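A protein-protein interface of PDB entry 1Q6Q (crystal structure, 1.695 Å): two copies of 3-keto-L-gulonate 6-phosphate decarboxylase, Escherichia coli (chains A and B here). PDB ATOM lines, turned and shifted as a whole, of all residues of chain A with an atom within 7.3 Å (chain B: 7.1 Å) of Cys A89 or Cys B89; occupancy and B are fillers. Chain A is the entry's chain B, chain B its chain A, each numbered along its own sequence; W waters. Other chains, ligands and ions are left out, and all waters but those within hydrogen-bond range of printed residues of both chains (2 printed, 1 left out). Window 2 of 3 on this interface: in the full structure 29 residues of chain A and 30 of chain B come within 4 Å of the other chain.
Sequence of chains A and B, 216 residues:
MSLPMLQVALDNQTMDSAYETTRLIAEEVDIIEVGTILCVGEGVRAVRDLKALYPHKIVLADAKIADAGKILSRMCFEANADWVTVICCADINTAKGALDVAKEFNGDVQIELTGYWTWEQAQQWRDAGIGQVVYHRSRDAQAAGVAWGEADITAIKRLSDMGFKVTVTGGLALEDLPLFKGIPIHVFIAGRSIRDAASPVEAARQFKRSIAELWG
Water W2 bridges the side-chain carboxylate of Glu A112 (2.6 Å) and the backbone carbonyl oxygen of Ala B66 (3.3 Å). Water W1 bridges O of Cys A89 (2.8 Å) and N of Tyr B116 (2.8 Å).
Hydrophobic or aromatic side chains of chain B that line the printed part of chain A: Ile B87 and Tyr B116. Of the 18 printed residues of chain A, 5 touch a printed residue of chain B. Printed residues of chain A that touch a printed residue of chain B: Ala A66, Ile A87, Cys A89, Tyr A116 and Gln A121.
Ala A66 touches Ile B87, but with the chains exchanged Ile A87 does not touch Ala B66 (4.9 Å). Ile A87 touches its own counterpart, Ile B87. Cys B89 touches its own counterpart, Cys A89. Cys A89 touches Thr B114, but with the chains exchanged Thr A114 does not touch Cys B89 (4.1 Å). 17 positions are printed for both chains. Of the 7 pairs that touch across the chains among the printed residues, 4 have their exchanged pair printed and touching as well.
The backbone carbonyl oxygen (O) of Ile B65 lies within hydrogen-bond range of the backbone NH (N) of Ile B87 (2.9 Å). The backbone NH of Thr B114 is in hydrogen-bond range of the side-chain sulfur of Cys B88, at 3.3 Å. NE2 of Gln B121 is in hydrogen-bond range of O of Cys B88 (3.1 Å). The backbone carbonyl oxygen (O) of Ile A65 is in hydrogen-bond range of the backbone NH (N) of Ile A87, 3.0 Å away. O of Cys A88 is in hydrogen-bond range of NE2 of Gln A121 (3.1 Å).
The side-chain sulfur (SG) of Cys B89 is disulfide-bonded to the side-chain sulfur (SG) of Cys A89 (2.1 Å).
Of the printed residues of chain B, Ala A66 touches Ile B87 (3.4 Å). Printed residues of chain B within 4 Å of Cys A89: Ile B87 (3.9 Å), Cys B89 (2.1 Å) and Thr B114 (3.6 Å). Gly A115 touches none of the printed residues of chain B. Printed residues of chain B within 4 Å of Tyr A116: Gln B121. Printed residues of chain A within 4 Å of Ile B87: Ala A66 (3.4 Å), Ile A87 (3.3 Å) and Cys A89 (3.9 Å). Of the printed residues of chain A, Cys B89 touches Cys A89. Of the printed residues of chain A, Tyr B116 touches Gln A121 (3.9 Å). Of the printed residues of chain A, Gln B121 touches Tyr A116. The nearest residue of chain B that does not touch Cys A89 is Gly B115 (4.6 Å). The nearest residue of chain A that does not touch Cys B89 is Thr A114 (4.1 Å).
Ile B87 touches Ala A66. Ile B87 touches Ile A87. Ile B87 touches Cys A89 (CG1 to SG, 3.9 Å). Cys A89 touches Thr B114. Gln B121 touches Tyr A116. Tyr B116 touches Gln A121.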
ATOM      1  N   ILE A  65     -23.988  19.707  -9.449  1.00  0.00           N
ATOM      2  CA  ILE A  65     -22.891  20.668  -9.624  1.00  0.00           C
ATOM      3  C   ILE A  65     -22.691  21.411  -8.309  1.00  0.00           C
ATOM      4  O   ILE A  65     -23.632  21.985  -7.809  1.00  0.00           O
ATOM      5  CB  ILE A  65     -23.225  21.604 -10.751  1.00  0.00           C
ATOM      6  CG1 ILE A  65     -23.280  20.859 -12.086  1.00  0.00           C
ATOM      7  CG2 ILE A  65     -22.192  22.766 -10.834  1.00  0.00           C
ATOM      8  CD1 ILE A  65     -23.960  21.618 -13.187  1.00  0.00           C
ATOM      9  N   ALA A  66     -21.446  21.396  -7.805  1.00  0.00           N
ATOM     10  CA  ALA A  66     -21.100  22.026  -6.544  1.00  0.00           C
ATOM     11  C   ALA A  66     -20.151  23.258  -6.710  1.00  0.00           C
ATOM     12  O   ALA A  66     -19.930  24.015  -5.734  1.00  0.00           O
ATOM     13  CB  ALA A  66     -20.447  20.991  -5.682  1.00  0.00           C
ATOM     14  N   VAL A  86     -27.921  21.515  -9.567  1.00  0.00           N
ATOM     15  CA  VAL A  86     -26.874  22.216  -8.807  1.00  0.00           C
ATOM     16  C   VAL A  86     -27.246  21.994  -7.343  1.00  0.00           C
ATOM     17  O   VAL A  86     -28.414  22.196  -6.946  1.00  0.00           O
ATOM     18  CB  VAL A  86     -26.904  23.732  -9.107  1.00  0.00           C
ATOM     19  CG1 VAL A  86     -25.974  24.467  -8.119  1.00  0.00           C
ATOM     20  CG2 VAL A  86     -26.534  24.003 -10.525  1.00  0.00           C
ATOM     21  N   ILE A  87     -26.292  21.568  -6.555  1.00  0.00           N
ATOM     22  CA  ILE A  87     -26.567  21.312  -5.146  1.00  0.00           C
ATOM     23  C   ILE A  87     -26.657  22.620  -4.354  1.00  0.00           C
ATOM     24  O   ILE A  87     -26.026  23.631  -4.703  1.00  0.00           O
ATOM     25  CB  ILE A  87     -25.583  20.379  -4.534  1.00  0.00           C
ATOM     26  CG1 ILE A  87     -24.163  20.916  -4.636  1.00  0.00           C
ATOM     27  CG2 ILE A  87     -25.722  19.093  -5.147  1.00  0.00           C
ATOM     28  CD1 ILE A  87     -23.341  20.467  -3.640  1.00  0.00           C
ATOM     29  N   CYS A  88     -27.506  22.608  -3.337  1.00  0.00           N
ATOM     30  CA  CYS A  88     -27.814  23.821  -2.611  1.00  0.00           C
ATOM     31  C   CYS A  88     -26.612  24.399  -1.843  1.00  0.00           C
ATOM     32  O   CYS A  88     -26.629  25.582  -1.570  1.00  0.00           O
ATOM     33  CB  CYS A  88     -29.026  23.620  -1.675  1.00  0.00           C
ATOM     34  SG  CYS A  88     -28.751  22.357  -0.496  1.00  0.00           S
ATOM     35  N   CYS A  89     -25.623  23.602  -1.482  1.00  0.00           N
ATOM     36  CA  CYS A  89     -24.468  24.127  -0.737  1.00  0.00           C
ATOM     37  C   CYS A  89     -23.442  24.796  -1.662  1.00  0.00           C
ATOM     38  O   CYS A  89     -22.370  25.205  -1.179  1.00  0.00           O
ATOM     39  CB  CYS A  89     -23.768  23.099   0.183  1.00  0.00           C
ATOM     40  SG  CYS A  89     -23.037  21.486  -0.341  1.00  0.00           S
ATOM     41  N   ALA A  90     -23.752  24.878  -2.970  1.00  0.00           N
ATOM     42  CA  ALA A  90     -22.894  25.591  -3.938  1.00  0.00           C
ATOM     43  C   ALA A  90     -23.006  27.094  -3.722  1.00  0.00           C
ATOM     44  O   ALA A  90     -24.056  27.629  -3.367  1.00  0.00           O
ATOM     45  CB  ALA A  90     -23.302  25.257  -5.370  1.00  0.00           C
ATOM     46  N   ASP A  91     -21.926  27.808  -4.014  1.00  0.00           N
ATOM     47  CA  ASP A  91     -21.994  29.275  -4.112  1.00  0.00           C
ATOM     48  C   ASP A  91     -23.132  29.758  -4.996  1.00  0.00           C
ATOM     49  O   ASP A  91     -23.421  29.185  -6.058  1.00  0.00           O
ATOM     50  CB  ASP A  91     -20.624  29.786  -4.629  1.00  0.00           C
ATOM     51  CG  ASP A  91     -20.403  31.245  -4.319  1.00  0.00           C
ATOM     52  OD1 ASP A  91     -19.937  31.536  -3.217  1.00  0.00           O
ATOM     53  OD2 ASP A  91     -20.800  32.148  -5.055  1.00  0.00           O
ATOM     54  N   ILE A  92     -23.826  30.821  -4.618  1.00  0.00           N
ATOM     55  CA  ILE A  92     -24.882  31.358  -5.445  1.00  0.00           C
ATOM     56  C   ILE A  92     -24.394  31.675  -6.856  1.00  0.00           C
ATOM     57  O   ILE A  92     -25.146  31.578  -7.823  1.00  0.00           O
ATOM     58  CB  ILE A  92     -25.510  32.601  -4.759  1.00  0.00           C
ATOM     59  CG1 ILE A  92     -26.659  33.146  -5.583  1.00  0.00           C
ATOM     60  CG2 ILE A  92     -24.434  33.722  -4.628  1.00  0.00           C
ATOM     61  CD1 ILE A  92     -27.878  32.189  -5.812  1.00  0.00           C
ATOM     62  N   THR A  94     -22.240  29.885  -8.513  1.00  0.00           N
ATOM     63  CA  THR A  94     -22.277  28.575  -9.183  1.00  0.00           C
ATOM     64  C   THR A  94     -23.648  28.356  -9.789  1.00  0.00           C
ATOM     65  O   THR A  94     -23.752  28.025 -10.943  1.00  0.00           O
ATOM     66  CB  THR A  94     -21.888  27.433  -8.210  1.00  0.00           C
ATOM     67  OG1 THR A  94     -20.561  27.634  -7.727  1.00  0.00           O
ATOM     68  CG2 THR A  94     -21.914  26.049  -8.945  1.00  0.00           C
ATOM     69  N   ILE A 111     -32.161  23.400  -8.234  1.00  0.00           N
ATOM     70  CA  ILE A 111     -31.404  23.302  -6.994  1.00  0.00           C
ATOM     71  C   ILE A 111     -31.816  22.078  -6.222  1.00  0.00           C
ATOM     72  O   ILE A 111     -33.001  21.886  -5.877  1.00  0.00           O
ATOM     73  CB  ILE A 111     -31.576  24.589  -6.114  1.00  0.00           C
ATOM     74  CG1 ILE A 111     -31.088  25.820  -6.884  1.00  0.00           C
ATOM     75  CG2 ILE A 111     -30.941  24.397  -4.788  1.00  0.00           C
ATOM     76  CD1 ILE A 111     -29.619  25.831  -7.273  1.00  0.00           C
ATOM     77  N   GLU A 112     -30.855  21.228  -5.948  1.00  0.00           N
ATOM     78  CA  GLU A 112     -31.105  20.104  -5.116  1.00  0.00           C
ATOM     79  C   GLU A 112     -31.081  20.510  -3.638  1.00  0.00           C
ATOM     80  O   GLU A 112     -30.031  20.929  -3.123  1.00  0.00           O
ATOM     81  CB  GLU A 112     -30.085  19.044  -5.310  1.00  0.00           C
ATOM     82  CG  GLU A 112     -30.435  17.837  -4.446  1.00  0.00           C
ATOM     83  CD  GLU A 112     -29.344  16.835  -4.459  1.00  0.00           C
ATOM     84  OE1 GLU A 112     -29.258  16.086  -5.484  1.00  0.00           O
ATOM     85  OE2 GLU A 112     -28.570  16.833  -3.476  1.00  0.00           O
ATOM     86  N   THR A 114     -31.145  19.496   0.032  1.00  0.00           N
ATOM     87  CA  THR A 114     -30.832  18.465   0.984  1.00  0.00           C
ATOM     88  C   THR A 114     -30.057  19.010   2.211  1.00  0.00           C
ATOM     89  O   THR A 114     -29.350  20.020   2.127  1.00  0.00           O
ATOM     90  CB  THR A 114     -30.048  17.366   0.251  1.00  0.00           C
ATOM     91  OG1 THR A 114     -30.249  16.103   0.929  1.00  0.00           O
ATOM     92  CG2 THR A 114     -28.525  17.645   0.241  1.00  0.00           C
ATOM     93  N   GLY A 115     -30.184  18.317   3.341  1.00  0.00           N
ATOM     94  CA  GLY A 115     -29.498  18.727   4.561  1.00  0.00           C
ATOM     95  C   GLY A 115     -29.825  20.164   4.909  1.00  0.00           C
ATOM     96  O   GLY A 115     -30.988  20.559   4.834  1.00  0.00           O
ATOM     97  N   TYR A 116     -28.809  20.962   5.221  1.00  0.00           N
ATOM     98  CA  TYR A 116     -29.053  22.331   5.696  1.00  0.00           C
ATOM     99  C   TYR A 116     -29.154  23.344   4.543  1.00  0.00           C
ATOM    100  O   TYR A 116     -28.309  23.395   3.638  1.00  0.00           O
ATOM    101  CB  TYR A 116     -27.995  22.754   6.725  1.00  0.00           C
ATOM    102  CG  TYR A 116     -27.588  21.658   7.749  1.00  0.00           C
ATOM    103  CD1 TYR A 116     -26.340  21.014   7.661  1.00  0.00           C
ATOM    104  CD2 TYR A 116     -28.450  21.272   8.802  1.00  0.00           C
ATOM    105  CE1 TYR A 116     -25.959  20.016   8.582  1.00  0.00           C
ATOM    106  CE2 TYR A 116     -28.070  20.274   9.734  1.00  0.00           C
ATOM    107  CZ  TYR A 116     -26.821  19.649   9.607  1.00  0.00           C
ATOM    108  OH  TYR A 116     -26.426  18.667  10.503  1.00  0.00           O
ATOM    109  N   TRP A 117     -30.221  24.126   4.559  1.00  0.00           N
ATOM    110  CA  TRP A 117     -30.390  25.226   3.634  1.00  0.00           C
ATOM    111  C   TRP A 117     -31.313  26.229   4.328  1.00  0.00           C
ATOM    112  O   TRP A 117     -31.889  25.904   5.345  1.00  0.00           O
ATOM    113  CB  TRP A 117     -30.915  24.744   2.251  1.00  0.00           C
ATOM    114  CG  TRP A 117     -32.177  23.892   2.291  1.00  0.00           C
ATOM    115  CD1 TRP A 117     -32.248  22.535   2.455  1.00  0.00           C
ATOM    116  CD2 TRP A 117     -33.524  24.350   2.157  1.00  0.00           C
ATOM    117  NE1 TRP A 117     -33.567  22.130   2.465  1.00  0.00           N
ATOM    118  CE2 TRP A 117     -34.369  23.223   2.270  1.00  0.00           C
ATOM    119  CE3 TRP A 117     -34.114  25.607   1.986  1.00  0.00           C
ATOM    120  CZ2 TRP A 117     -35.761  23.319   2.208  1.00  0.00           C
ATOM    121  CZ3 TRP A 117     -35.509  25.701   1.911  1.00  0.00           C
ATOM    122  CH2 TRP A 117     -36.317  24.558   2.025  1.00  0.00           C
ATOM    123  N   GLN A 121     -31.471  31.646   1.396  1.00  0.00           N
ATOM    124  CA  GLN A 121     -30.993  30.979   0.171  1.00  0.00           C
ATOM    125  C   GLN A 121     -32.080  30.852  -0.850  1.00  0.00           C
ATOM    126  O   GLN A 121     -31.849  31.118  -2.031  1.00  0.00           O
ATOM    127  CB  GLN A 121     -30.459  29.595   0.475  1.00  0.00           C
ATOM    128  CG  GLN A 121     -29.148  29.598   1.199  1.00  0.00           C
ATOM    129  CD  GLN A 121     -28.485  28.256   1.180  1.00  0.00           C
ATOM    130  OE1 GLN A 121     -28.646  27.466   2.115  1.00  0.00           O
ATOM    131  NE2 GLN A 121     -27.711  27.990   0.125  1.00  0.00           N
ATOM    132  N   TRP A 125     -32.199  32.185  -4.683  1.00  0.00           N
ATOM    133  CA  TRP A 125     -32.433  31.386  -5.901  1.00  0.00           C
ATOM    134  C   TRP A 125     -33.541  31.981  -6.698  1.00  0.00           C
ATOM    135  O   TRP A 125     -33.379  32.188  -7.887  1.00  0.00           O
ATOM    136  CB  TRP A 125     -32.681  29.870  -5.599  1.00  0.00           C
ATOM    137  CG  TRP A 125     -31.569  29.222  -4.855  1.00  0.00           C
ATOM    138  CD1 TRP A 125     -30.224  29.433  -5.046  1.00  0.00           C
ATOM    139  CD2 TRP A 125     -31.672  28.319  -3.760  1.00  0.00           C
ATOM    140  NE1 TRP A 125     -29.504  28.710  -4.137  1.00  0.00           N
ATOM    141  CE2 TRP A 125     -30.371  28.022  -3.333  1.00  0.00           C
ATOM    142  CE3 TRP A 125     -32.753  27.679  -3.109  1.00  0.00           C
ATOM    143  CZ2 TRP A 125     -30.105  27.149  -2.303  1.00  0.00           C
ATOM    144  CZ3 TRP A 125     -32.489  26.837  -2.081  1.00  0.00           C
ATOM    145  CH2 TRP A 125     -31.181  26.583  -1.665  1.00  0.00           C
ATOM    146  N   ILE B  65     -19.059  13.430  -3.713  1.00  0.00           N
ATOM    147  CA  ILE B  65     -20.175  12.549  -3.379  1.00  0.00           C
ATOM    148  C   ILE B  65     -21.135  13.249  -2.417  1.00  0.00           C
ATOM    149  O   ILE B  65     -20.724  13.760  -1.348  1.00  0.00           O
ATOM    150  CB  ILE B  65     -19.624  11.282  -2.759  1.00  0.00           C
ATOM    151  CG1 ILE B  65     -18.875  10.463  -3.807  1.00  0.00           C
ATOM    152  CG2 ILE B  65     -20.733  10.406  -2.136  1.00  0.00           C
ATOM    153  CD1 ILE B  65     -18.047   9.303  -3.264  1.00  0.00           C
ATOM    154  N   ALA B  66     -22.405  13.338  -2.799  1.00  0.00           N
ATOM    155  CA  ALA B  66     -23.421  14.034  -2.019  1.00  0.00           C
ATOM    156  C   ALA B  66     -24.494  13.112  -1.441  1.00  0.00           C
ATOM    157  O   ALA B  66     -25.253  13.539  -0.593  1.00  0.00           O
ATOM    158  CB  ALA B  66     -24.075  15.045  -2.890  1.00  0.00           C
ATOM    159  N   VAL B  86     -16.149  13.598  -0.393  1.00  0.00           N
ATOM    160  CA  VAL B  86     -17.561  13.728  -0.073  1.00  0.00           C
ATOM    161  C   VAL B  86     -17.817  15.160   0.298  1.00  0.00           C
ATOM    162  O   VAL B  86     -17.041  15.749   1.061  1.00  0.00           O
ATOM    163  CB  VAL B  86     -17.880  12.862   1.119  1.00  0.00           C
ATOM    164  CG1 VAL B  86     -19.315  13.123   1.629  1.00  0.00           C
ATOM    165  CG2 VAL B  86     -17.651  11.369   0.743  1.00  0.00           C
ATOM    166  N   ILE B  87     -18.881  15.729  -0.236  1.00  0.00           N
ATOM    167  CA  ILE B  87     -19.202  17.121   0.009  1.00  0.00           C
ATOM    168  C   ILE B  87     -19.773  17.290   1.435  1.00  0.00           C
ATOM    169  O   ILE B  87     -20.474  16.392   1.948  1.00  0.00           O
ATOM    170  CB  ILE B  87     -20.104  17.635  -1.109  1.00  0.00           C
ATOM    171  CG1 ILE B  87     -20.057  19.118  -1.235  1.00  0.00           C
ATOM    172  CG2 ILE B  87     -21.543  17.230  -0.958  1.00  0.00           C
ATOM    173  CD1 ILE B  87     -20.390  19.457  -2.642  1.00  0.00           C
ATOM    174  N   CYS B  88     -19.410  18.406   2.066  1.00  0.00           N
ATOM    175  CA  CYS B  88     -19.781  18.673   3.468  1.00  0.00           C
ATOM    176  C   CYS B  88     -21.298  18.710   3.712  1.00  0.00           C
ATOM    177  O   CYS B  88     -21.738  18.392   4.811  1.00  0.00           O
ATOM    178  CB  CYS B  88     -19.112  19.977   3.988  1.00  0.00           C
ATOM    179  SG  CYS B  88     -19.506  21.436   3.060  1.00  0.00           S
ATOM    180  N   CYS B  89     -22.116  19.085   2.729  1.00  0.00           N
ATOM    181  CA  CYS B  89     -23.559  19.075   2.970  1.00  0.00           C
ATOM    182  C   CYS B  89     -24.224  17.734   2.786  1.00  0.00           C
ATOM    183  O   CYS B  89     -25.444  17.653   2.949  1.00  0.00           O
ATOM    184  CB  CYS B  89     -24.292  20.107   2.150  1.00  0.00           C
ATOM    185  SG  CYS B  89     -24.209  19.915   0.403  1.00  0.00           S
ATOM    186  N   ALA B  90     -23.456  16.676   2.489  1.00  0.00           N
ATOM    187  CA  ALA B  90     -24.008  15.329   2.514  1.00  0.00           C
ATOM    188  C   ALA B  90     -24.467  14.969   3.927  1.00  0.00           C
ATOM    189  O   ALA B  90     -23.887  15.414   4.928  1.00  0.00           O
ATOM    190  CB  ALA B  90     -22.997  14.356   2.056  1.00  0.00           C
ATOM    191  N   ASP B  91     -25.487  14.128   4.009  1.00  0.00           N
ATOM    192  CA  ASP B  91     -25.817  13.490   5.259  1.00  0.00           C
ATOM    193  C   ASP B  91     -24.591  12.864   5.899  1.00  0.00           C
ATOM    194  O   ASP B  91     -23.769  12.236   5.251  1.00  0.00           O
ATOM    195  CB  ASP B  91     -26.850  12.385   4.981  1.00  0.00           C
ATOM    196  CG  ASP B  91     -27.495  11.849   6.249  1.00  0.00           C
ATOM    197  OD1 ASP B  91     -28.496  12.451   6.680  1.00  0.00           O
ATOM    198  OD2 ASP B  91     -27.053  10.873   6.873  1.00  0.00           O
ATOM    199  N   ILE B  92     -24.475  12.917   7.230  1.00  0.00           N
ATOM    200  CA  ILE B  92     -23.394  12.202   7.876  1.00  0.00           C
ATOM    201  C   ILE B  92     -23.270  10.743   7.523  1.00  0.00           C
ATOM    202  O   ILE B  92     -22.173  10.225   7.463  1.00  0.00           O
ATOM    203  CB  ILE B  92     -23.480  12.413   9.469  1.00  0.00           C
ATOM    204  CG1 ILE B  92     -22.224  11.884  10.170  1.00  0.00           C
ATOM    205  CG2 ILE B  92     -24.714  11.735  10.008  1.00  0.00           C
ATOM    206  CD1 ILE B  92     -20.972  12.594   9.839  1.00  0.00           C
ATOM    207  N   ILE B 111     -13.550  15.175   3.374  1.00  0.00           N
ATOM    208  CA  ILE B 111     -14.732  16.062   3.289  1.00  0.00           C
ATOM    209  C   ILE B 111     -14.364  17.374   2.612  1.00  0.00           C
ATOM    210  O   ILE B 111     -13.484  18.115   3.086  1.00  0.00           O
ATOM    211  CB  ILE B 111     -15.314  16.370   4.734  1.00  0.00           C
ATOM    212  CG1 ILE B 111     -15.796  15.105   5.425  1.00  0.00           C
ATOM    213  CG2 ILE B 111     -16.424  17.365   4.589  1.00  0.00           C
ATOM    214  CD1 ILE B 111     -16.814  14.388   4.670  1.00  0.00           C
ATOM    215  N   GLU B 112     -15.065  17.696   1.513  1.00  0.00           N
ATOM    216  CA  GLU B 112     -14.908  18.979   0.847  1.00  0.00           C
ATOM    217  C   GLU B 112     -15.701  20.062   1.576  1.00  0.00           C
ATOM    218  O   GLU B 112     -16.928  19.989   1.679  1.00  0.00           O
ATOM    219  CB  GLU B 112     -15.369  18.925  -0.606  1.00  0.00           C
ATOM    220  CG  GLU B 112     -15.090  20.297  -1.205  1.00  0.00           C
ATOM    221  CD  GLU B 112     -15.719  20.550  -2.536  1.00  0.00           C
ATOM    222  OE1 GLU B 112     -15.137  20.087  -3.537  1.00  0.00           O
ATOM    223  OE2 GLU B 112     -16.771  21.239  -2.580  1.00  0.00           O
ATOM    224  N   THR B 114     -17.273  23.504   1.692  1.00  0.00           N
ATOM    225  CA  THR B 114     -17.777  24.520   0.792  1.00  0.00           C
ATOM    226  C   THR B 114     -18.938  25.325   1.388  1.00  0.00           C
ATOM    227  O   THR B 114     -19.941  24.768   1.832  1.00  0.00           O
ATOM    228  CB  THR B 114     -18.148  23.867  -0.583  1.00  0.00           C
ATOM    229  OG1 THR B 114     -18.811  24.825  -1.411  1.00  0.00           O
ATOM    230  CG2 THR B 114     -19.172  22.709  -0.452  1.00  0.00           C
ATOM    231  N   GLY B 115     -18.780  26.652   1.368  1.00  0.00           N
ATOM    232  CA  GLY B 115     -19.835  27.556   1.794  1.00  0.00           C
ATOM    233  C   GLY B 115     -20.191  27.261   3.238  1.00  0.00           C
ATOM    234  O   GLY B 115     -19.296  27.254   4.077  1.00  0.00           O
ATOM    235  N   TYR B 116     -21.459  26.958   3.515  1.00  0.00           N
ATOM    236  CA  TYR B 116     -21.921  26.808   4.905  1.00  0.00           C
ATOM    237  C   TYR B 116     -21.645  25.403   5.386  1.00  0.00           C
ATOM    238  O   TYR B 116     -21.975  24.405   4.742  1.00  0.00           O
ATOM    239  CB  TYR B 116     -23.399  27.193   5.080  1.00  0.00           C
ATOM    240  CG  TYR B 116     -23.784  28.485   4.336  1.00  0.00           C
ATOM    241  CD1 TYR B 116     -24.719  28.459   3.284  1.00  0.00           C
ATOM    242  CD2 TYR B 116     -23.215  29.723   4.674  1.00  0.00           C
ATOM    243  CE1 TYR B 116     -25.079  29.621   2.591  1.00  0.00           C
ATOM    244  CE2 TYR B 116     -23.579  30.895   3.989  1.00  0.00           C
ATOM    245  CZ  TYR B 116     -24.510  30.829   2.944  1.00  0.00           C
ATOM    246  OH  TYR B 116     -24.877  31.966   2.249  1.00  0.00           O
ATOM    247  N   TRP B 117     -20.921  25.350   6.481  1.00  0.00           N
ATOM    248  CA  TRP B 117     -20.762  24.161   7.251  1.00  0.00           C
ATOM    249  C   TRP B 117     -20.526  24.673   8.689  1.00  0.00           C
ATOM    250  O   TRP B 117     -20.288  25.861   8.861  1.00  0.00           O
ATOM    251  CB  TRP B 117     -19.605  23.302   6.693  1.00  0.00           C
ATOM    252  CG  TRP B 117     -18.320  24.050   6.514  1.00  0.00           C
ATOM    253  CD1 TRP B 117     -17.934  24.745   5.428  1.00  0.00           C
ATOM    254  CD2 TRP B 117     -17.232  24.164   7.471  1.00  0.00           C
ATOM    255  NE1 TRP B 117     -16.701  25.322   5.636  1.00  0.00           N
ATOM    256  CE2 TRP B 117     -16.240  24.958   6.879  1.00  0.00           C
ATOM    257  CE3 TRP B 117     -17.016  23.678   8.766  1.00  0.00           C
ATOM    258  CZ2 TRP B 117     -15.042  25.305   7.554  1.00  0.00           C
ATOM    259  CZ3 TRP B 117     -15.811  23.986   9.422  1.00  0.00           C
ATOM    260  CH2 TRP B 117     -14.854  24.779   8.814  1.00  0.00           C
ATOM    261  N   GLN B 121     -20.743  20.122  12.815  1.00  0.00           N
ATOM    262  CA  GLN B 121     -20.538  19.100  11.784  1.00  0.00           C
ATOM    263  C   GLN B 121     -19.092  18.574  11.794  1.00  0.00           C
ATOM    264  O   GLN B 121     -18.871  17.384  11.636  1.00  0.00           O
ATOM    265  CB  GLN B 121     -20.815  19.640  10.399  1.00  0.00           C
ATOM    266  CG  GLN B 121     -22.235  19.944   9.987  1.00  0.00           C
ATOM    267  CD  GLN B 121     -22.258  20.275   8.538  1.00  0.00           C
ATOM    268  OE1 GLN B 121     -22.017  21.424   8.166  1.00  0.00           O
ATOM    269  NE2 GLN B 121     -22.482  19.268   7.687  1.00  0.00           N
ATOM    270  N   TRP B 125     -17.713  14.769  12.025  1.00  0.00           N
ATOM    271  CA  TRP B 125     -16.804  14.078  11.084  1.00  0.00           C
ATOM    272  C   TRP B 125     -15.668  13.389  11.813  1.00  0.00           C
ATOM    273  O   TRP B 125     -15.398  12.232  11.564  1.00  0.00           O
ATOM    274  CB  TRP B 125     -16.270  14.998   9.963  1.00  0.00           C
ATOM    275  CG  TRP B 125     -17.330  15.599   9.108  1.00  0.00           C
ATOM    276  CD1 TRP B 125     -18.476  14.999   8.660  1.00  0.00           C
ATOM    277  CD2 TRP B 125     -17.388  16.942   8.652  1.00  0.00           C
ATOM    278  NE1 TRP B 125     -19.218  15.891   7.931  1.00  0.00           N
ATOM    279  CE2 TRP B 125     -18.574  17.097   7.928  1.00  0.00           C
ATOM    280  CE3 TRP B 125     -16.499  18.013   8.705  1.00  0.00           C
ATOM    281  CZ2 TRP B 125     -18.918  18.267   7.335  1.00  0.00           C
ATOM    282  CZ3 TRP B 125     -16.847  19.165   8.182  1.00  0.00           C
ATOM    283  CH2 TRP B 125     -18.059  19.314   7.491  1.00  0.00           C
HETATM  284  O   HOH W   1     -23.066  26.462   1.238  1.00  0.00           O
HETATM  285  O   HOH W   2     -27.783  14.638  -2.371  1.00  0.00           O
